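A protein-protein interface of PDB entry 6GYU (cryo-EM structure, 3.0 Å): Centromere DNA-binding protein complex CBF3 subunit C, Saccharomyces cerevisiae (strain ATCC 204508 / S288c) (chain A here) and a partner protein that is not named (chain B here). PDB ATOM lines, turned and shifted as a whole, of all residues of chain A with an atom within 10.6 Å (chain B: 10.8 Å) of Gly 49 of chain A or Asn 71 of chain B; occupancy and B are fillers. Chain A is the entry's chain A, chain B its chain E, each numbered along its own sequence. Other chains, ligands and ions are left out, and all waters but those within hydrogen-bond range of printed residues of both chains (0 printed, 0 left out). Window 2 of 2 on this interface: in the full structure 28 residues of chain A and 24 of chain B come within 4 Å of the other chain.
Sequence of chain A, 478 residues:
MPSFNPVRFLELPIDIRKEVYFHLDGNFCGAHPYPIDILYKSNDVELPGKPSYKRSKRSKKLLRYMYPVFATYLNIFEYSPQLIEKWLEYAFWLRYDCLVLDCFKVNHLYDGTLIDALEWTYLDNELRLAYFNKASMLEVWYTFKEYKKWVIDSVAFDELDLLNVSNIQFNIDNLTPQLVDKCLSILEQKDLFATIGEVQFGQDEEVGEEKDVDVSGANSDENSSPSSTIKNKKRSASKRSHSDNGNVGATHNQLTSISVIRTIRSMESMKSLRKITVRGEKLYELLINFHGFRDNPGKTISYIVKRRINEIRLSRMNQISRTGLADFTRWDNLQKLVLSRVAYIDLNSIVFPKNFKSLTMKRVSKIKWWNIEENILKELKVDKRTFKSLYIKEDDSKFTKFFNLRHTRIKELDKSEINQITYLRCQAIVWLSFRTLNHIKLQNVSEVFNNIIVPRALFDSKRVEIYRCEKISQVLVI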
ATOM      1  N   ASN A  43      -2.924  11.099  14.675  1.00  0.00           N
ATOM      2  CA  ASN A  43      -3.695  11.638  15.787  1.00  0.00           C
ATOM      3  C   ASN A  43      -4.255  13.011  15.437  1.00  0.00           C
ATOM      4  O   ASN A  43      -5.462  13.247  15.537  1.00  0.00           O
ATOM      5  CB  ASN A  43      -2.827  11.706  17.044  1.00  0.00           C
ATOM      6  N   ASP A  44      -3.391  13.917  14.989  1.00  0.00           N
ATOM      7  CA  ASP A  44      -3.777  15.294  14.741  1.00  0.00           C
ATOM      8  C   ASP A  44      -4.578  15.420  13.444  1.00  0.00           C
ATOM      9  O   ASP A  44      -4.576  14.535  12.586  1.00  0.00           O
ATOM     10  CB  ASP A  44      -2.540  16.188  14.686  1.00  0.00           C
ATOM     11  N   VAL A  45      -5.279  16.545  13.319  1.00  0.00           N
ATOM     12  CA  VAL A  45      -6.037  16.899  12.124  1.00  0.00           C
ATOM     13  C   VAL A  45      -5.505  18.237  11.633  1.00  0.00           C
ATOM     14  O   VAL A  45      -5.744  19.269  12.271  1.00  0.00           O
ATOM     15  CB  VAL A  45      -7.544  16.995  12.401  1.00  0.00           C
ATOM     16  CG1 VAL A  45      -8.290  17.399  11.141  1.00  0.00           C
ATOM     17  CG2 VAL A  45      -8.077  15.695  12.951  1.00  0.00           C
ATOM     18  N   GLU A  46      -4.795  18.222  10.507  1.00  0.00           N
ATOM     19  CA  GLU A  46      -4.163  19.434   9.995  1.00  0.00           C
ATOM     20  C   GLU A  46      -5.217  20.418   9.504  1.00  0.00           C
ATOM     21  O   GLU A  46      -6.063  20.075   8.670  1.00  0.00           O
ATOM     22  CB  GLU A  46      -3.185  19.091   8.877  1.00  0.00           C
ATOM     23  CG  GLU A  46      -1.957  18.330   9.342  1.00  0.00           C
ATOM     24  CD  GLU A  46      -1.004  18.015   8.207  1.00  0.00           C
ATOM     25  OE1 GLU A  46      -1.357  18.291   7.042  1.00  0.00           O
ATOM     26  OE2 GLU A  46       0.096  17.490   8.478  1.00  0.00           O
ATOM     27  N   LEU A  47      -5.170  21.636  10.030  1.00  0.00           N
ATOM     28  CA  LEU A  47      -6.138  22.683   9.768  1.00  0.00           C
ATOM     29  C   LEU A  47      -5.463  23.908   9.158  1.00  0.00           C
ATOM     30  O   LEU A  47      -4.255  24.106   9.322  1.00  0.00           O
ATOM     31  CB  LEU A  47      -6.848  23.094  11.063  1.00  0.00           C
ATOM     32  CG  LEU A  47      -7.750  22.042  11.691  1.00  0.00           C
ATOM     33  CD1 LEU A  47      -8.219  22.537  13.030  1.00  0.00           C
ATOM     34  CD2 LEU A  47      -8.928  21.761  10.783  1.00  0.00           C
ATOM     35  N   PRO A  48      -6.211  24.737   8.431  1.00  0.00           N
ATOM     36  CA  PRO A  48      -5.648  26.009   7.959  1.00  0.00           C
ATOM     37  C   PRO A  48      -5.489  27.025   9.077  1.00  0.00           C
ATOM     38  O   PRO A  48      -6.044  26.855  10.167  1.00  0.00           O
ATOM     39  CB  PRO A  48      -6.679  26.482   6.928  1.00  0.00           C
ATOM     40  CG  PRO A  48      -7.405  25.251   6.528  1.00  0.00           C
ATOM     41  CD  PRO A  48      -7.471  24.411   7.745  1.00  0.00           C
ATOM     42  N   GLY A  49      -4.740  28.091   8.813  1.00  0.00           N
ATOM     43  CA  GLY A  49      -4.570  29.162   9.777  1.00  0.00           C
ATOM     44  C   GLY A  49      -3.643  28.821  10.925  1.00  0.00           C
ATOM     45  O   GLY A  49      -3.718  29.430  11.992  1.00  0.00           O
ATOM     46  N   ARG A  55      -2.473  34.646   5.478  1.00  0.00           N
ATOM     47  CA  ARG A  55      -2.375  35.927   4.788  1.00  0.00           C
ATOM     48  C   ARG A  55      -1.347  35.863   3.664  1.00  0.00           C
ATOM     49  O   ARG A  55      -0.267  35.298   3.831  1.00  0.00           O
ATOM     50  CB  ARG A  55      -2.012  37.040   5.773  1.00  0.00           C
ATOM     51  N   GLU A  78     -10.529  22.617  -0.439  1.00  0.00           N
ATOM     52  CA  GLU A  78     -10.621  23.851   0.328  1.00  0.00           C
ATOM     53  C   GLU A  78     -10.072  23.710   1.738  1.00  0.00           C
ATOM     54  O   GLU A  78      -9.733  24.723   2.357  1.00  0.00           O
ATOM     55  CB  GLU A  78     -12.066  24.345   0.385  1.00  0.00           C
ATOM     56  CG  GLU A  78     -12.571  24.907  -0.922  1.00  0.00           C
ATOM     57  CD  GLU A  78     -11.887  26.204  -1.292  1.00  0.00           C
ATOM     58  OE1 GLU A  78     -11.545  26.982  -0.378  1.00  0.00           O
ATOM     59  OE2 GLU A  78     -11.684  26.444  -2.498  1.00  0.00           O
ATOM     60  N   TYR A  79      -9.995  22.491   2.266  1.00  0.00           N
ATOM     61  CA  TYR A  79      -9.152  22.261   3.425  1.00  0.00           C
ATOM     62  C   TYR A  79      -7.703  22.485   3.014  1.00  0.00           C
ATOM     63  O   TYR A  79      -7.276  22.036   1.945  1.00  0.00           O
ATOM     64  CB  TYR A  79      -9.361  20.843   3.978  1.00  0.00           C
ATOM     65  CG  TYR A  79      -8.852  19.722   3.099  1.00  0.00           C
ATOM     66  CD1 TYR A  79      -9.620  19.227   2.056  1.00  0.00           C
ATOM     67  CD2 TYR A  79      -7.608  19.145   3.328  1.00  0.00           C
ATOM     68  CE1 TYR A  79      -9.152  18.208   1.253  1.00  0.00           C
ATOM     69  CE2 TYR A  79      -7.135  18.131   2.532  1.00  0.00           C
ATOM     70  CZ  TYR A  79      -7.911  17.665   1.501  1.00  0.00           C
ATOM     71  OH  TYR A  79      -7.436  16.651   0.713  1.00  0.00           O
ATOM     72  N   SER A  80      -6.962  23.211   3.858  1.00  0.00           N
ATOM     73  CA  SER A  80      -5.586  23.644   3.620  1.00  0.00           C
ATOM     74  C   SER A  80      -5.440  24.373   2.287  1.00  0.00           C
ATOM     75  O   SER A  80      -4.957  23.779   1.315  1.00  0.00           O
ATOM     76  CB  SER A  80      -4.621  22.455   3.684  1.00  0.00           C
ATOM     77  OG  SER A  80      -3.294  22.859   3.398  1.00  0.00           O
ATOM     78  N   PRO A  81      -5.869  25.636   2.182  1.00  0.00           N
ATOM     79  CA  PRO A  81      -5.700  26.377   0.922  1.00  0.00           C
ATOM     80  C   PRO A  81      -4.260  26.751   0.602  1.00  0.00           C
ATOM     81  O   PRO A  81      -4.024  27.384  -0.432  1.00  0.00           O
ATOM     82  CB  PRO A  81      -6.552  27.632   1.141  1.00  0.00           C
ATOM     83  CG  PRO A  81      -6.521  27.837   2.599  1.00  0.00           C
ATOM     84  CD  PRO A  81      -6.504  26.471   3.214  1.00  0.00           C
ATOM     85  N   GLN A  82      -3.297  26.404   1.461  1.00  0.00           N
ATOM     86  CA  GLN A  82      -1.896  26.419   1.063  1.00  0.00           C
ATOM     87  C   GLN A  82      -1.630  25.432  -0.065  1.00  0.00           C
ATOM     88  O   GLN A  82      -0.736  25.661  -0.883  1.00  0.00           O
ATOM     89  CB  GLN A  82      -1.006  26.102   2.262  1.00  0.00           C
ATOM     90  CG  GLN A  82      -1.041  27.156   3.350  1.00  0.00           C
ATOM     91  CD  GLN A  82      -0.165  26.796   4.531  1.00  0.00           C
ATOM     92  OE1 GLN A  82       0.433  25.720   4.569  1.00  0.00           O
ATOM     93  NE2 GLN A  82      -0.085  27.694   5.504  1.00  0.00           N
ATOM     94  N   LEU A  83      -2.391  24.336  -0.125  1.00  0.00           N
ATOM     95  CA  LEU A  83      -2.302  23.403  -1.240  1.00  0.00           C
ATOM     96  C   LEU A  83      -2.808  24.012  -2.541  1.00  0.00           C
ATOM     97  O   LEU A  83      -2.366  23.593  -3.611  1.00  0.00           O
ATOM     98  CB  LEU A  83      -3.075  22.121  -0.897  1.00  0.00           C
ATOM     99  CG  LEU A  83      -3.006  20.820  -1.712  1.00  0.00           C
ATOM    100  CD1 LEU A  83      -3.953  20.763  -2.910  1.00  0.00           C
ATOM    101  CD2 LEU A  83      -1.579  20.578  -2.162  1.00  0.00           C
ATOM    102  N   LYS B  46     -13.662  15.579   3.731  1.00  0.00           N
ATOM    103  CA  LYS B  46     -12.650  16.223   4.561  1.00  0.00           C
ATOM    104  C   LYS B  46     -12.761  17.741   4.501  1.00  0.00           C
ATOM    105  O   LYS B  46     -12.544  18.408   5.515  1.00  0.00           O
ATOM    106  CB  LYS B  46     -11.248  15.773   4.151  1.00  0.00           C
ATOM    107  CG  LYS B  46     -10.162  16.277   5.087  1.00  0.00           C
ATOM    108  CD  LYS B  46      -8.803  15.721   4.762  1.00  0.00           C
ATOM    109  CE  LYS B  46      -7.755  16.346   5.662  1.00  0.00           C
ATOM    110  NZ  LYS B  46      -7.961  15.965   7.084  1.00  0.00           N
ATOM    111  N   THR B  50     -13.644  19.803   7.766  1.00  0.00           N
ATOM    112  CA  THR B  50     -12.703  20.865   8.085  1.00  0.00           C
ATOM    113  C   THR B  50     -13.433  22.179   8.328  1.00  0.00           C
ATOM    114  O   THR B  50     -13.057  22.931   9.233  1.00  0.00           O
ATOM    115  CB  THR B  50     -11.674  21.000   6.963  1.00  0.00           C
ATOM    116  OG1 THR B  50     -11.027  19.737   6.771  1.00  0.00           O
ATOM    117  CG2 THR B  50     -10.613  22.027   7.310  1.00  0.00           C
ATOM    118  N   ILE B  53     -14.695  21.701  11.895  1.00  0.00           N
ATOM    119  CA  ILE B  53     -13.708  21.854  12.959  1.00  0.00           C
ATOM    120  C   ILE B  53     -13.240  23.307  13.057  1.00  0.00           C
ATOM    121  O   ILE B  53     -12.976  23.814  14.157  1.00  0.00           O
ATOM    122  CB  ILE B  53     -12.547  20.864  12.747  1.00  0.00           C
ATOM    123  CG1 ILE B  53     -13.059  19.431  12.856  1.00  0.00           C
ATOM    124  CG2 ILE B  53     -11.497  21.009  13.805  1.00  0.00           C
ATOM    125  CD1 ILE B  53     -12.075  18.392  12.378  1.00  0.00           C
ATOM    126  N   GLN B  54     -13.184  24.019  11.924  1.00  0.00           N
ATOM    127  CA  GLN B  54     -12.948  25.461  11.967  1.00  0.00           C
ATOM    128  C   GLN B  54     -14.061  26.199  12.693  1.00  0.00           C
ATOM    129  O   GLN B  54     -13.786  27.130  13.458  1.00  0.00           O
ATOM    130  CB  GLN B  54     -12.811  26.032  10.558  1.00  0.00           C
ATOM    131  CG  GLN B  54     -11.510  25.744   9.856  1.00  0.00           C
ATOM    132  CD  GLN B  54     -11.503  26.309   8.455  1.00  0.00           C
ATOM    133  OE1 GLN B  54     -12.511  26.830   7.981  1.00  0.00           O
ATOM    134  NE2 GLN B  54     -10.365  26.220   7.785  1.00  0.00           N
ATOM    135  N   TRP B  55     -15.315  25.792  12.475  1.00  0.00           N
ATOM    136  CA  TRP B  55     -16.424  26.411  13.193  1.00  0.00           C
ATOM    137  C   TRP B  55     -16.374  26.093  14.681  1.00  0.00           C
ATOM    138  O   TRP B  55     -16.719  26.938  15.512  1.00  0.00           O
ATOM    139  CB  TRP B  55     -17.752  25.952  12.609  1.00  0.00           C
ATOM    140  CG  TRP B  55     -18.906  26.538  13.322  1.00  0.00           C
ATOM    141  CD1 TRP B  55     -19.345  27.824  13.255  1.00  0.00           C
ATOM    142  CD2 TRP B  55     -19.738  25.878  14.274  1.00  0.00           C
ATOM    143  NE1 TRP B  55     -20.429  27.998  14.080  1.00  0.00           N
ATOM    144  CE2 TRP B  55     -20.686  26.815  14.719  1.00  0.00           C
ATOM    145  CE3 TRP B  55     -19.781  24.580  14.783  1.00  0.00           C
ATOM    146  CZ2 TRP B  55     -21.664  26.494  15.645  1.00  0.00           C
ATOM    147  CZ3 TRP B  55     -20.752  24.264  15.698  1.00  0.00           C
ATOM    148  CH2 TRP B  55     -21.680  25.215  16.120  1.00  0.00           C
ATOM    149  N   CYS B  56     -15.955  24.875  15.035  1.00  0.00           N
ATOM    150  CA  CYS B  56     -15.805  24.528  16.442  1.00  0.00           C
ATOM    151  C   CYS B  56     -14.654  25.274  17.103  1.00  0.00           C
ATOM    152  O   CYS B  56     -14.727  25.556  18.303  1.00  0.00           O
ATOM    153  CB  CYS B  56     -15.609  23.021  16.603  1.00  0.00           C
ATOM    154  SG  CYS B  56     -17.070  22.027  16.238  1.00  0.00           S
ATOM    155  N   GLN B  57     -13.601  25.608  16.357  1.00  0.00           N
ATOM    156  CA  GLN B  57     -12.522  26.392  16.950  1.00  0.00           C
ATOM    157  C   GLN B  57     -12.873  27.870  17.059  1.00  0.00           C
ATOM    158  O   GLN B  57     -12.489  28.522  18.036  1.00  0.00           O
ATOM    159  CB  GLN B  57     -11.222  26.226  16.164  1.00  0.00           C
ATOM    160  CG  GLN B  57     -10.496  24.928  16.430  1.00  0.00           C
ATOM    161  CD  GLN B  57      -9.142  24.895  15.758  1.00  0.00           C
ATOM    162  OE1 GLN B  57      -8.811  25.774  14.964  1.00  0.00           O
ATOM    163  NE2 GLN B  57      -8.331  23.909  16.111  1.00  0.00           N
ATOM    164  N   LEU B  58     -13.594  28.428  16.086  1.00  0.00           N
ATOM    165  CA  LEU B  58     -13.943  29.843  16.158  1.00  0.00           C
ATOM    166  C   LEU B  58     -15.109  30.113  17.103  1.00  0.00           C
ATOM    167  O   LEU B  58     -15.468  31.278  17.306  1.00  0.00           O
ATOM    168  CB  LEU B  58     -14.245  30.407  14.760  1.00  0.00           C
ATOM    169  CG  LEU B  58     -15.435  29.997  13.880  1.00  0.00           C
ATOM    170  CD1 LEU B  58     -16.688  30.847  14.115  1.00  0.00           C
ATOM    171  CD2 LEU B  58     -15.033  30.051  12.414  1.00  0.00           C
ATOM    172  N   ILE B  62     -14.047  23.333  20.841  1.00  0.00           N
ATOM    173  CA  ILE B  62     -12.811  22.598  21.072  1.00  0.00           C
ATOM    174  C   ILE B  62     -11.684  23.619  21.177  1.00  0.00           C
ATOM    175  O   ILE B  62     -11.678  24.597  20.427  1.00  0.00           O
ATOM    176  CB  ILE B  62     -12.530  21.550  19.976  1.00  0.00           C
ATOM    177  CG1 ILE B  62     -11.293  20.709  20.299  1.00  0.00           C
ATOM    178  CG2 ILE B  62     -12.497  22.145  18.558  1.00  0.00           C
ATOM    179  CD1 ILE B  62     -11.201  19.440  19.500  1.00  0.00           C
ATOM    180  N   PRO B  63     -10.782  23.499  22.152  1.00  0.00           N
ATOM    181  CA  PRO B  63      -9.744  24.525  22.316  1.00  0.00           C
ATOM    182  C   PRO B  63      -8.682  24.456  21.230  1.00  0.00           C
ATOM    183  O   PRO B  63      -8.287  23.377  20.784  1.00  0.00           O
ATOM    184  CB  PRO B  63      -9.154  24.213  23.696  1.00  0.00           C
ATOM    185  CG  PRO B  63     -10.229  23.475  24.409  1.00  0.00           C
ATOM    186  CD  PRO B  63     -10.905  22.655  23.354  1.00  0.00           C
ATOM    187  N   THR B  64      -8.230  25.633  20.804  1.00  0.00           N
ATOM    188  CA  THR B  64      -7.116  25.723  19.873  1.00  0.00           C
ATOM    189  C   THR B  64      -5.819  25.302  20.568  1.00  0.00           C
ATOM    190  O   THR B  64      -5.663  25.511  21.776  1.00  0.00           O
ATOM    191  CB  THR B  64      -7.014  27.152  19.312  1.00  0.00           C
ATOM    192  OG1 THR B  64      -5.913  27.254  18.400  1.00  0.00           O
ATOM    193  CG2 THR B  64      -6.881  28.197  20.420  1.00  0.00           C
ATOM    194  N   PRO B  65      -4.891  24.653  19.853  1.00  0.00           N
ATOM    195  CA  PRO B  65      -3.676  24.172  20.532  1.00  0.00           C
ATOM    196  C   PRO B  65      -2.671  25.267  20.846  1.00  0.00           C
ATOM    197  O   PRO B  65      -2.042  25.229  21.910  1.00  0.00           O
ATOM    198  CB  PRO B  65      -3.111  23.141  19.544  1.00  0.00           C
ATOM    199  CG  PRO B  65      -3.627  23.566  18.221  1.00  0.00           C
ATOM    200  CD  PRO B  65      -4.991  24.135  18.476  1.00  0.00           C
ATOM    201  N   GLU B  66      -2.502  26.246  19.959  1.00  0.00           N
ATOM    202  CA  GLU B  66      -1.520  27.298  20.175  1.00  0.00           C
ATOM    203  C   GLU B  66      -1.930  28.538  19.397  1.00  0.00           C
ATOM    204  O   GLU B  66      -3.055  28.644  18.902  1.00  0.00           O
ATOM    205  CB  GLU B  66      -0.112  26.855  19.760  1.00  0.00           C
ATOM    206  N   ASP B  67      -0.995  29.479  19.301  1.00  0.00           N
ATOM    207  CA  ASP B  67      -1.203  30.740  18.602  1.00  0.00           C
ATOM    208  C   ASP B  67      -0.140  30.901  17.524  1.00  0.00           C
ATOM    209  O   ASP B  67       1.059  30.821  17.819  1.00  0.00           O
ATOM    210  CB  ASP B  67      -1.157  31.920  19.574  1.00  0.00           C
ATOM    211  N   ASN B  68      -0.598  31.122  16.283  1.00  0.00           N
ATOM    212  CA  ASN B  68       0.249  31.310  15.095  1.00  0.00           C
ATOM    213  C   ASN B  68       1.187  30.126  14.865  1.00  0.00           C
ATOM    214  O   ASN B  68       2.404  30.282  14.755  1.00  0.00           O
ATOM    215  CB  ASN B  68       1.031  32.626  15.160  1.00  0.00           C
ATOM    216  CG  ASN B  68       0.142  33.840  14.987  1.00  0.00           C
ATOM    217  OD1 ASN B  68      -0.754  33.852  14.142  1.00  0.00           O
ATOM    218  ND2 ASN B  68       0.383  34.871  15.790  1.00  0.00           N
ATOM    219  N   SER B  69       0.610  28.930  14.794  1.00  0.00           N
ATOM    220  CA  SER B  69       1.363  27.718  14.502  1.00  0.00           C
ATOM    221  C   SER B  69       0.442  26.766  13.758  1.00  0.00           C
ATOM    222  O   SER B  69      -0.616  27.157  13.258  1.00  0.00           O
ATOM    223  CB  SER B  69       1.912  27.073  15.777  1.00  0.00           C
ATOM    224  OG  SER B  69       0.862  26.569  16.583  1.00  0.00           O
ATOM    225  N   VAL B  70       0.860  25.502  13.683  1.00  0.00           N
ATOM    226  CA  VAL B  70       0.027  24.493  13.045  1.00  0.00           C
ATOM    227  C   VAL B  70      -1.102  24.113  13.989  1.00  0.00           C
ATOM    228  O   VAL B  70      -0.907  23.352  14.945  1.00  0.00           O
ATOM    229  CB  VAL B  70       0.871  23.272  12.650  1.00  0.00           C
ATOM    230  CG1 VAL B  70       0.005  22.213  11.981  1.00  0.00           C
ATOM    231  CG2 VAL B  70       2.016  23.690  11.741  1.00  0.00           C
ATOM    232  N   ASN B  71      -2.286  24.668  13.745  1.00  0.00           N
ATOM    233  CA  ASN B  71      -3.476  24.335  14.514  1.00  0.00           C
ATOM    234  C   ASN B  71      -3.949  22.939  14.142  1.00  0.00           C
ATOM    235  O   ASN B  71      -4.182  22.644  12.967  1.00  0.00           O
ATOM    236  CB  ASN B  71      -4.585  25.381  14.318  1.00  0.00           C
ATOM    237  CG  ASN B  71      -4.799  25.757  12.864  1.00  0.00           C
ATOM    238  OD1 ASN B  71      -4.106  25.276  11.970  1.00  0.00           O
ATOM    239  ND2 ASN B  71      -5.773  26.625  12.623  1.00  0.00           N
ATOM    240  N   SER B  72      -4.058  22.074  15.143  1.00  0.00           N
ATOM    241  CA  SER B  72      -4.395  20.680  14.914  1.00  0.00           C
ATOM    242  C   SER B  72      -5.103  20.124  16.137  1.00  0.00           C
ATOM    243  O   SER B  72      -4.656  20.313  17.270  1.00  0.00           O
ATOM    244  CB  SER B  72      -3.150  19.842  14.604  1.00  0.00           C
ATOM    245  OG  SER B  72      -2.548  20.244  13.386  1.00  0.00           O
ATOM    246  N   VAL B  73      -6.207  19.437  15.895  1.00  0.00           N
ATOM    247  CA  VAL B  73      -7.000  18.806  16.946  1.00  0.00           C
ATOM    248  C   VAL B  73      -6.802  17.300  16.855  1.00  0.00           C
ATOM    249  O   VAL B  73      -6.578  16.782  15.754  1.00  0.00           O
ATOM    250  CB  VAL B  73      -8.493  19.178  16.845  1.00  0.00           C
ATOM    251  CG1 VAL B  73      -8.663  20.663  17.058  1.00  0.00           C
ATOM    252  CG2 VAL B  73      -9.072  18.786  15.502  1.00  0.00           C
ATOM    253  N   PRO B  74      -6.799  16.580  17.970  1.00  0.00           N
ATOM    254  CA  PRO B  74      -6.771  15.118  17.889  1.00  0.00           C
ATOM    255  C   PRO B  74      -8.152  14.567  17.587  1.00  0.00           C
ATOM    256  O   PRO B  74      -9.170  15.194  17.886  1.00  0.00           O
ATOM    257  CB  PRO B  74      -6.291  14.692  19.281  1.00  0.00           C
ATOM    258  CG  PRO B  74      -5.623  15.903  19.842  1.00  0.00           C
ATOM    259  CD  PRO B  74      -6.405  17.059  19.302  1.00  0.00           C
ATOM    260  N   LEU B  78     -12.522  15.056  19.872  1.00  0.00           N
ATOM    261  CA  LEU B  78     -13.247  15.941  18.970  1.00  0.00           C
ATOM    262  C   LEU B  78     -14.740  15.823  19.246  1.00  0.00           C
ATOM    263  O   LEU B  78     -15.320  14.749  19.019  1.00  0.00           O
ATOM    264  CB  LEU B  78     -12.938  15.589  17.515  1.00  0.00           C
ATOM    265  CG  LEU B  78     -13.532  16.486  16.434  1.00  0.00           C
ATOM    266  CD1 LEU B  78     -13.012  17.899  16.579  1.00  0.00           C
ATOM    267  CD2 LEU B  78     -13.178  15.933  15.071  1.00  0.00           C
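Of the printed residues of chain A, Asn 71 of chain B touches Val 45, Leu 47, Pro 48 and Gly 49. Leu 47 of chain A touches just these residues of chain B: Thr 50 (3.9 Å), Ile 53 (3.7 Å), Gln 57 (3.4 Å) and Asn 71 (2.9 Å). No residue of chain A comes within 4 Å of Val 70 of chain B. Ser 72 of chain B touches just these residues of chain A: Asp 44, Val 45 and Glu 46. Of the printed residues of chain A, Ile 53 of chain B touches Leu 47. Of the printed residues of chain A, Gln 57 of chain B touches Leu 47 (3.4 Å). Of the printed residues of chain A, Lys 46 of chain B touches Tyr 79. Of the printed residues of chain B, Asn 43 of chain A touches Val 73 (3.7 Å) and Pro 74 (3.3 Å). Printed residues of chain B within 4 Å of Tyr 79 of chain A: Lys 46 (3.6 Å) and Thr 50 (3.4 Å). Ser 80 of chain A touches none of the printed residues of chain B. Pro 65 of chain B touches none of the printed residues of chain A. The nearest residue of chain A that does not touch Asn 71 of chain B is Glu 46 of chain A (4.2 Å). The nearest printed residue of chain A that does not touch Val 73 of chain B is Leu 47 of chain A (4.5 Å).
Of the 14 printed residues of chain A, 8 touch a printed residue of chain B. Hydrophobic or aromatic side chains of chain A that line the printed part of chain B: Val 45, Leu 47, Pro 48 and Tyr 79. Along chain A the printed residues that touch a printed residue of chain B span positions 43 to 79. Of the 22 printed residues of chain B, 9 touch a printed residue of chain A. Among the printed residues, 18 pairs touch across the chains. Among the printed residues, no Asp or Glu carboxylate lies within 4 Å of a Lys or Arg side-chain nitrogen of the other chain.
The backbone NH of Val 45 of chain A lies within hydrogen-bond range of the backbone carbonyl oxygen of Val 73 of chain B, 2.8 Å away. The side-chain amide oxygen of Asn 71 of chain B lies close to the backbone carbonyl oxygen of Leu 47 of chain A. The backbone carbonyl oxygen (O) of Pro 48 of chain A sits at hydrogen-bond distance from the side-chain amide nitrogen (ND2) of Asn 71 of chain B (2.5 Å).
Among the printed residues, pairs that only touch across the chains: Asn 43 of chain A with Pro 74 of chain B (3.3 Å), Val 45 of chain A with Ser 72 of chain B (3.3 Å), Asp 44 of chain A with Val 73 of chain B (3.3 Å), Pro 48 of chain A with Gln 54 of chain B (3.4 Å), Leu 47 of chain A with Gln 57 of chain B (3.4 Å), Tyr 79 of chain A with Thr 50 of chain B (3.4 Å), Gly 49 of chain A with Asn 71 of chain B (3.5 Å), Tyr 79 of chain A with Lys 46 of chain B (3.6 Å), Leu 47 of chain A with Ile 53 of chain B (3.7 Å), Asp 44 of chain A with Ser 72 of chain B (3.7 Å), Asn 43 of chain A with Val 73 of chain B (3.7 Å), Val 45 of chain A with Asn 71 of chain B (3.8 Å), Glu 46 of chain A with Ser 72 of chain B (3.8 Å), Leu 47 of chain A with Thr 50 of chain B (3.9 Å) and Pro 48 of chain A with Thr 50 of chain B (3.97 Å).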
